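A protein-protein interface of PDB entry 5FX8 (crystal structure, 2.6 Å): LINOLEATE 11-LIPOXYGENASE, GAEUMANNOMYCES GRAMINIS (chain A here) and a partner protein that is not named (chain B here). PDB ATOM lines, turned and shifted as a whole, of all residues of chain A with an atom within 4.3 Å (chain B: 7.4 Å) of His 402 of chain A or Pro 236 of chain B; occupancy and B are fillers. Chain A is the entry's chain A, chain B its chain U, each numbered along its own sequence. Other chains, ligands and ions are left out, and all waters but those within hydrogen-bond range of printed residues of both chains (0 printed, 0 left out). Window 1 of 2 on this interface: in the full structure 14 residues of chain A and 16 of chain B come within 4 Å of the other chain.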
ATOM      1  N   TYR A 398      19.122 -14.078  34.647  1.00  0.00           N
ATOM      2  CA  TYR A 398      18.990 -14.045  33.202  1.00  0.00           C
ATOM      3  C   TYR A 398      17.786 -13.214  32.775  1.00  0.00           C
ATOM      4  O   TYR A 398      17.845 -12.501  31.777  1.00  0.00           O
ATOM      5  CB  TYR A 398      18.892 -15.474  32.685  1.00  0.00           C
ATOM      6  CG  TYR A 398      18.822 -15.631  31.208  1.00  0.00           C
ATOM      7  CD1 TYR A 398      19.436 -14.728  30.365  1.00  0.00           C
ATOM      8  CD2 TYR A 398      18.134 -16.688  30.651  1.00  0.00           C
ATOM      9  CE1 TYR A 398      19.375 -14.877  29.040  1.00  0.00           C
ATOM     10  CE2 TYR A 398      18.064 -16.838  29.321  1.00  0.00           C
ATOM     11  CZ  TYR A 398      18.684 -15.934  28.517  1.00  0.00           C
ATOM     12  OH  TYR A 398      18.616 -16.069  27.164  1.00  0.00           O
ATOM     13  N   GLU A 399      16.686 -13.270  33.515  1.00  0.00           N
ATOM     14  CA  GLU A 399      15.496 -12.558  33.068  1.00  0.00           C
ATOM     15  C   GLU A 399      15.644 -11.060  33.283  1.00  0.00           C
ATOM     16  O   GLU A 399      15.391 -10.258  32.375  1.00  0.00           O
ATOM     17  CB  GLU A 399      14.265 -13.110  33.792  1.00  0.00           C
ATOM     18  CG  GLU A 399      13.971 -14.591  33.509  1.00  0.00           C
ATOM     19  CD  GLU A 399      13.433 -15.384  34.723  1.00  0.00           C
ATOM     20  OE1 GLU A 399      12.963 -14.785  35.721  1.00  0.00           O
ATOM     21  OE2 GLU A 399      13.462 -16.635  34.669  1.00  0.00           O
ATOM     22  N   ASP A 400      16.072 -10.667  34.481  1.00  0.00           N
ATOM     23  CA  ASP A 400      16.369  -9.260  34.729  1.00  0.00           C
ATOM     24  C   ASP A 400      17.454  -8.737  33.795  1.00  0.00           C
ATOM     25  O   ASP A 400      17.326  -7.637  33.249  1.00  0.00           O
ATOM     26  CB  ASP A 400      16.750  -9.072  36.193  1.00  0.00           C
ATOM     27  CG  ASP A 400      15.543  -9.053  37.081  1.00  0.00           C
ATOM     28  OD1 ASP A 400      14.456  -9.023  36.496  1.00  0.00           O
ATOM     29  OD2 ASP A 400      15.634  -9.051  38.328  1.00  0.00           O
ATOM     30  N   ALA A 401      18.508  -9.522  33.583  1.00  0.00           N
ATOM     31  CA  ALA A 401      19.582  -9.150  32.669  1.00  0.00           C
ATOM     32  C   ALA A 401      19.075  -8.993  31.243  1.00  0.00           C
ATOM     33  O   ALA A 401      19.467  -8.068  30.529  1.00  0.00           O
ATOM     34  CB  ALA A 401      20.708 -10.189  32.710  1.00  0.00           C
ATOM     35  N   HIS A 402      18.232  -9.907  30.803  1.00  0.00           N
ATOM     36  CA  HIS A 402      17.699  -9.827  29.462  1.00  0.00           C
ATOM     37  C   HIS A 402      16.887  -8.558  29.274  1.00  0.00           C
ATOM     38  O   HIS A 402      17.021  -7.881  28.251  1.00  0.00           O
ATOM     39  CB  HIS A 402      16.866 -11.061  29.174  1.00  0.00           C
ATOM     40  CG  HIS A 402      16.099 -10.961  27.903  1.00  0.00           C
ATOM     41  ND1 HIS A 402      16.667 -11.220  26.672  1.00  0.00           N
ATOM     42  CD2 HIS A 402      14.819 -10.592  27.664  1.00  0.00           C
ATOM     43  CE1 HIS A 402      15.763 -11.023  25.732  1.00  0.00           C
ATOM     44  NE2 HIS A 402      14.637 -10.638  26.306  1.00  0.00           N
ATOM     45  N   ARG A 403      16.070  -8.187  30.260  1.00  0.00           N
ATOM     46  CA  ARG A 403      15.326  -6.940  30.118  1.00  0.00           C
ATOM     47  C   ARG A 403      16.267  -5.743  30.040  1.00  0.00           C
ATOM     48  O   ARG A 403      16.209  -4.949  29.088  1.00  0.00           O
ATOM     49  CB  ARG A 403      14.325  -6.766  31.252  1.00  0.00           C
ATOM     50  CG  ARG A 403      13.303  -7.824  31.289  1.00  0.00           C
ATOM     51  CD  ARG A 403      12.358  -7.628  32.455  1.00  0.00           C
ATOM     52  NE  ARG A 403      11.611  -8.851  32.762  1.00  0.00           N
ATOM     53  CZ  ARG A 403      10.451  -9.202  32.211  1.00  0.00           C
ATOM     54  NH1 ARG A 403       9.871  -8.438  31.310  1.00  0.00           N
ATOM     55  NH2 ARG A 403       9.868 -10.328  32.571  1.00  0.00           N
ATOM     56  N   LEU A 404      17.149  -5.596  31.034  1.00  0.00           N
ATOM     57  CA  LEU A 404      17.992  -4.405  31.082  1.00  0.00           C
ATOM     58  C   LEU A 404      18.888  -4.309  29.850  1.00  0.00           C
ATOM     59  O   LEU A 404      18.997  -3.248  29.226  1.00  0.00           O
ATOM     60  CB  LEU A 404      18.818  -4.398  32.357  1.00  0.00           C
ATOM     61  CG  LEU A 404      19.776  -3.212  32.506  1.00  0.00           C
ATOM     62  CD1 LEU A 404      19.061  -1.839  32.559  1.00  0.00           C
ATOM     63  CD2 LEU A 404      20.669  -3.431  33.713  1.00  0.00           C
ATOM     64  N   ILE A 405      19.536  -5.415  29.482  1.00  0.00           N
ATOM     65  CA  ILE A 405      20.377  -5.417  28.295  1.00  0.00           C
ATOM     66  C   ILE A 405      19.564  -5.066  27.068  1.00  0.00           C
ATOM     67  O   ILE A 405      20.067  -4.392  26.167  1.00  0.00           O
ATOM     68  CB  ILE A 405      21.086  -6.761  28.133  1.00  0.00           C
ATOM     69  CG1 ILE A 405      22.155  -6.914  29.207  1.00  0.00           C
ATOM     70  CG2 ILE A 405      21.743  -6.854  26.813  1.00  0.00           C
ATOM     71  CD1 ILE A 405      22.928  -8.242  29.195  1.00  0.00           C
ATOM     72  N   GLY A 406      18.295  -5.481  27.014  1.00  0.00           N
ATOM     73  CA  GLY A 406      17.440  -5.047  25.921  1.00  0.00           C
ATOM     74  C   GLY A 406      17.316  -3.539  25.837  1.00  0.00           C
ATOM     75  O   GLY A 406      17.402  -2.955  24.761  1.00  0.00           O
ATOM     76  N   THR B 177       4.512  -7.951  30.873  1.00  0.00           N
ATOM     77  CA  THR B 177       5.776  -8.531  31.319  1.00  0.00           C
ATOM     78  C   THR B 177       5.921 -10.016  31.010  1.00  0.00           C
ATOM     79  O   THR B 177       7.037 -10.467  30.741  1.00  0.00           O
ATOM     80  CB  THR B 177       5.967  -8.330  32.836  1.00  0.00           C
ATOM     81  OG1 THR B 177       5.035  -9.135  33.564  1.00  0.00           O
ATOM     82  CG2 THR B 177       5.744  -6.881  33.205  1.00  0.00           C
ATOM     83  N   ASN B 178       4.836 -10.787  31.029  1.00  0.00           N
ATOM     84  CA  ASN B 178       4.917 -12.198  30.700  1.00  0.00           C
ATOM     85  C   ASN B 178       3.754 -12.599  29.805  1.00  0.00           C
ATOM     86  O   ASN B 178       2.658 -12.047  29.882  1.00  0.00           O
ATOM     87  CB  ASN B 178       4.950 -13.056  31.960  1.00  0.00           C
ATOM     88  CG  ASN B 178       6.149 -12.756  32.806  1.00  0.00           C
ATOM     89  OD1 ASN B 178       6.179 -11.754  33.512  1.00  0.00           O
ATOM     90  ND2 ASN B 178       7.159 -13.610  32.730  1.00  0.00           N
ATOM     91  N   ILE B 179       4.022 -13.565  28.938  1.00  0.00           N
ATOM     92  CA  ILE B 179       3.050 -14.054  27.981  1.00  0.00           C
ATOM     93  C   ILE B 179       3.091 -15.569  27.983  1.00  0.00           C
ATOM     94  O   ILE B 179       4.144 -16.163  27.739  1.00  0.00           O
ATOM     95  CB  ILE B 179       3.324 -13.527  26.568  1.00  0.00           C
ATOM     96  CG1 ILE B 179       3.305 -12.005  26.573  1.00  0.00           C
ATOM     97  CG2 ILE B 179       2.305 -14.102  25.621  1.00  0.00           C
ATOM     98  CD1 ILE B 179       3.570 -11.381  25.235  1.00  0.00           C
ATOM     99  N   TYR B 197       8.460 -16.319  15.660  1.00  0.00           N
ATOM    100  CA  TYR B 197       7.797 -15.135  16.171  1.00  0.00           C
ATOM    101  C   TYR B 197       8.463 -13.912  15.573  1.00  0.00           C
ATOM    102  O   TYR B 197       9.553 -13.983  15.017  1.00  0.00           O
ATOM    103  CB  TYR B 197       7.807 -15.087  17.705  1.00  0.00           C
ATOM    104  CG  TYR B 197       9.113 -14.628  18.320  1.00  0.00           C
ATOM    105  CD1 TYR B 197      10.146 -15.525  18.564  1.00  0.00           C
ATOM    106  CD2 TYR B 197       9.304 -13.298  18.665  1.00  0.00           C
ATOM    107  CE1 TYR B 197      11.337 -15.109  19.115  1.00  0.00           C
ATOM    108  CE2 TYR B 197      10.477 -12.872  19.215  1.00  0.00           C
ATOM    109  CZ  TYR B 197      11.505 -13.777  19.446  1.00  0.00           C
ATOM    110  OH  TYR B 197      12.691 -13.334  20.010  1.00  0.00           O
ATOM    111  N   VAL B 199       8.401  -9.301  16.131  1.00  0.00           N
ATOM    112  CA  VAL B 199       7.924  -8.130  16.848  1.00  0.00           C
ATOM    113  C   VAL B 199       7.981  -6.953  15.887  1.00  0.00           C
ATOM    114  O   VAL B 199       9.063  -6.586  15.423  1.00  0.00           O
ATOM    115  CB  VAL B 199       8.757  -7.839  18.107  1.00  0.00           C
ATOM    116  CG1 VAL B 199       8.127  -6.735  18.897  1.00  0.00           C
ATOM    117  CG2 VAL B 199       8.898  -9.066  18.971  1.00  0.00           C
ATOM    118  N   ILE B 227      11.761 -14.983  13.674  1.00  0.00           N
ATOM    119  CA  ILE B 227      12.766 -15.608  14.520  1.00  0.00           C
ATOM    120  C   ILE B 227      12.261 -16.997  14.890  1.00  0.00           C
ATOM    121  O   ILE B 227      11.247 -17.125  15.574  1.00  0.00           O
ATOM    122  CB  ILE B 227      13.043 -14.766  15.777  1.00  0.00           C
ATOM    123  CG1 ILE B 227      13.581 -13.398  15.381  1.00  0.00           C
ATOM    124  CG2 ILE B 227      14.012 -15.464  16.719  1.00  0.00           C
ATOM    125  CD1 ILE B 227      13.584 -12.445  16.502  1.00  0.00           C
ATOM    126  N   SER B 233      16.422 -22.070  22.164  1.00  0.00           N
ATOM    127  CA  SER B 233      16.308 -20.627  22.136  1.00  0.00           C
ATOM    128  C   SER B 233      16.187 -20.064  23.549  1.00  0.00           C
ATOM    129  O   SER B 233      15.626 -20.690  24.449  1.00  0.00           O
ATOM    130  CB  SER B 233      15.140 -20.205  21.254  1.00  0.00           C
ATOM    131  OG  SER B 233      13.985 -20.904  21.591  1.00  0.00           O
ATOM    132  N   GLY B 234      16.773 -18.892  23.747  1.00  0.00           N
ATOM    133  CA  GLY B 234      16.727 -18.198  25.006  1.00  0.00           C
ATOM    134  C   GLY B 234      15.706 -17.084  25.015  1.00  0.00           C
ATOM    135  O   GLY B 234      14.805 -17.014  24.173  1.00  0.00           O
ATOM    136  N   LEU B 235      15.844 -16.208  25.987  1.00  0.00           N
ATOM    137  CA  LEU B 235      14.858 -15.183  26.188  1.00  0.00           C
ATOM    138  C   LEU B 235      14.723 -14.329  24.936  1.00  0.00           C
ATOM    139  O   LEU B 235      15.712 -14.073  24.265  1.00  0.00           O
ATOM    140  CB  LEU B 235      15.223 -14.363  27.403  1.00  0.00           C
ATOM    141  CG  LEU B 235      15.002 -15.164  28.688  1.00  0.00           C
ATOM    142  CD1 LEU B 235      15.582 -14.428  29.861  1.00  0.00           C
ATOM    143  CD2 LEU B 235      13.524 -15.416  28.903  1.00  0.00           C
ATOM    144  N   PRO B 236      13.503 -13.870  24.615  1.00  0.00           N
ATOM    145  CA  PRO B 236      12.274 -13.824  25.400  1.00  0.00           C
ATOM    146  C   PRO B 236      11.548 -15.138  25.613  1.00  0.00           C
ATOM    147  O   PRO B 236      10.650 -15.156  26.432  1.00  0.00           O
ATOM    148  CB  PRO B 236      11.402 -12.883  24.580  1.00  0.00           C
ATOM    149  CG  PRO B 236      11.836 -13.067  23.246  1.00  0.00           C
ATOM    150  CD  PRO B 236      13.309 -13.199  23.328  1.00  0.00           C
ATOM    151  N   VAL B 237      11.924 -16.201  24.911  1.00  0.00           N
ATOM    152  CA  VAL B 237      11.279 -17.497  25.094  1.00  0.00           C
ATOM    153  C   VAL B 237      11.606 -18.028  26.484  1.00  0.00           C
ATOM    154  O   VAL B 237      12.767 -18.297  26.792  1.00  0.00           O
ATOM    155  CB  VAL B 237      11.734 -18.479  24.010  1.00  0.00           C
ATOM    156  CG1 VAL B 237      11.206 -19.853  24.268  1.00  0.00           C
ATOM    157  CG2 VAL B 237      11.263 -18.017  22.698  1.00  0.00           C
ATOM    158  N   GLU B 238      10.582 -18.205  27.319  1.00  0.00           N
ATOM    159  CA  GLU B 238      10.762 -18.850  28.613  1.00  0.00           C
ATOM    160  C   GLU B 238      10.573 -20.363  28.574  1.00  0.00           C
ATOM    161  O   GLU B 238      11.187 -21.073  29.375  1.00  0.00           O
ATOM    162  CB  GLU B 238       9.784 -18.299  29.646  1.00  0.00           C
ATOM    163  CG  GLU B 238       9.773 -16.835  29.813  1.00  0.00           C
ATOM    164  CD  GLU B 238       8.935 -16.431  31.007  1.00  0.00           C
ATOM    165  OE1 GLU B 238       7.694 -16.272  30.860  1.00  0.00           O
ATOM    166  OE2 GLU B 238       9.522 -16.292  32.105  1.00  0.00           O
ATOM    167  N   SER B 239       9.709 -20.876  27.703  1.00  0.00           N
ATOM    168  CA  SER B 239       9.448 -22.309  27.644  1.00  0.00           C
ATOM    169  C   SER B 239       8.777 -22.629  26.323  1.00  0.00           C
ATOM    170  O   SER B 239       8.097 -21.780  25.750  1.00  0.00           O
ATOM    171  CB  SER B 239       8.565 -22.743  28.799  1.00  0.00           C
ATOM    172  OG  SER B 239       7.423 -21.926  28.776  1.00  0.00           O
ATOM    173  N   SER B 250       5.909 -19.702  26.103  1.00  0.00           N
ATOM    174  CA  SER B 250       5.932 -18.626  27.088  1.00  0.00           C
ATOM    175  C   SER B 250       6.982 -17.576  26.747  1.00  0.00           C
ATOM    176  O   SER B 250       8.041 -17.881  26.204  1.00  0.00           O
ATOM    177  CB  SER B 250       6.232 -19.146  28.484  1.00  0.00           C
ATOM    178  OG  SER B 250       5.269 -20.070  28.880  1.00  0.00           O
ATOM    179  N   PHE B 251       6.705 -16.342  27.126  1.00  0.00           N
ATOM    180  CA  PHE B 251       7.591 -15.234  26.820  1.00  0.00           C
ATOM    181  C   PHE B 251       7.764 -14.343  28.040  1.00  0.00           C
ATOM    182  O   PHE B 251       6.812 -14.065  28.766  1.00  0.00           O
ATOM    183  CB  PHE B 251       7.058 -14.378  25.679  1.00  0.00           C
ATOM    184  CG  PHE B 251       7.150 -14.999  24.318  1.00  0.00           C
ATOM    185  CD1 PHE B 251       8.322 -14.915  23.577  1.00  0.00           C
ATOM    186  CD2 PHE B 251       6.038 -15.596  23.736  1.00  0.00           C
ATOM    187  CE1 PHE B 251       8.393 -15.446  22.298  1.00  0.00           C
ATOM    188  CE2 PHE B 251       6.107 -16.129  22.467  1.00  0.00           C
ATOM    189  CZ  PHE B 251       7.281 -16.051  21.748  1.00  0.00           C
ATOM    190  N   ALA B 252       8.982 -13.893  28.262  1.00  0.00           N
ATOM    191  CA  ALA B 252       9.279 -12.876  29.261  1.00  0.00           C
ATOM    192  C   ALA B 252      10.059 -11.794  28.557  1.00  0.00           C
ATOM    193  O   ALA B 252      11.045 -12.082  27.881  1.00  0.00           O
ATOM    194  CB  ALA B 252      10.098 -13.423  30.426  1.00  0.00           C
ATOM    195  N   GLY B 253       9.610 -10.567  28.671  1.00  0.00           N
ATOM    196  CA  GLY B 253      10.302  -9.516  27.963  1.00  0.00           C
ATOM    197  C   GLY B 253       9.463  -8.268  27.984  1.00  0.00           C
ATOM    198  O   GLY B 253       8.366  -8.232  28.533  1.00  0.00           O
ATOM    199  N   GLU B 254      10.007  -7.249  27.387  1.00  0.00           N
ATOM    200  CA  GLU B 254       9.404  -5.938  27.428  1.00  0.00           C
ATOM    201  C   GLU B 254       8.757  -5.718  26.075  1.00  0.00           C
ATOM    202  O   GLU B 254       9.442  -5.571  25.061  1.00  0.00           O
ATOM    203  CB  GLU B 254      10.448  -4.874  27.752  1.00  0.00           C
ATOM    204  CG  GLU B 254      11.219  -5.093  29.070  1.00  0.00           C
ATOM    205  CD  GLU B 254      10.414  -4.703  30.313  1.00  0.00           C
ATOM    206  OE1 GLU B 254      10.352  -3.503  30.651  1.00  0.00           O
ATOM    207  OE2 GLU B 254       9.825  -5.588  30.949  1.00  0.00           O
ATOM    208  N   LEU B 261       3.691  -8.425  19.262  1.00  0.00           N
ATOM    209  CA  LEU B 261       4.314  -9.739  19.162  1.00  0.00           C
ATOM    210  C   LEU B 261       3.426 -10.680  18.358  1.00  0.00           C
ATOM    211  O   LEU B 261       2.258 -10.867  18.690  1.00  0.00           O
ATOM    212  CB  LEU B 261       4.545 -10.342  20.548  1.00  0.00           C
ATOM    213  CG  LEU B 261       5.021 -11.789  20.541  1.00  0.00           C
ATOM    214  CD1 LEU B 261       6.357 -11.830  19.940  1.00  0.00           C
ATOM    215  CD2 LEU B 261       5.109 -12.297  21.925  1.00  0.00           C
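N of Leu 235 of chain B is in hydrogen-bond range of OH of Tyr 398 of chain A (3.0 Å). The backbone carbonyl oxygen (O) of Thr 177 of chain B is in hydrogen-bond range of the guanidinium group (NH2) of Arg 403 of chain A, at 3.4 Å. NH1 of Arg 403 of chain A is in salt-bridge range of OE2 of Glu 254 of chain B (2.9 Å). The guanidinium group of Arg 403 of chain A sits at hydrogen-bond distance from the backbone carbonyl oxygen of Gly 253 of chain B, 3.2 Å away.
The side-chain hydroxyl of Thr 177 of chain B sits at hydrogen-bond distance from the side-chain amide oxygen of Asn 178 of chain B (2.9 Å). N of Ala 252 of chain B is in hydrogen-bond range of O of Pro 236 of chain B (2.8 Å). O of Thr 177 of chain B is in hydrogen-bond range of N of Gly 253 of chain B (3.3 Å).
His 402 of chain A touches just these residues of chain B: Leu 235 and Pro 236. Pro 236 of chain B touches just one residue of chain A: His 402. Of the printed residues of chain A, Thr 177 of chain B touches Arg 403 (3.4 Å). Of the printed residues of chain B, Tyr 398 of chain A touches Gly 234 (3.6 Å) and Leu 235 (3.0 Å). Of the printed residues of chain B, Arg 403 of chain A touches Thr 177 (3.4 Å), Ala 252 (3.8 Å), Gly 253 (3.2 Å) and Glu 254 (2.9 Å). Printed residues of chain A within 4 Å of Gly 234 of chain B: Tyr 398 (3.6 Å). Of the printed residues of chain A, Ala 252 of chain B touches Arg 403. Phe 251 of chain B touches none of the printed residues of chain A. Asn 178 of chain B touches none of the printed residues of chain A.
Hydrophobic or aromatic side chains of chain A within 4 Å of the printed part of chain B: Tyr 398 and His 402. Of the 19 printed residues of chain B, 7 touch a printed residue of chain A. Printed residues of chain B that touch a printed residue of chain A: Thr 177, Gly 234, Leu 235, Pro 236, Ala 252, Gly 253 and Glu 254. Hydrophobic or aromatic side chains of chain B that line the printed part of chain A: Leu 235 and Ala 252.
Among the printed residues, pairs that only touch across the chains: His 402 of chain A with Leu 235 of chain B, Tyr 398 of chain A with Gly 234 of chain B, Glu 399 of chain A with Leu 235 of chain B, Arg 403 of chain A with Ala 252 of chain B and His 402 of chain A with Pro 236 of chain B.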
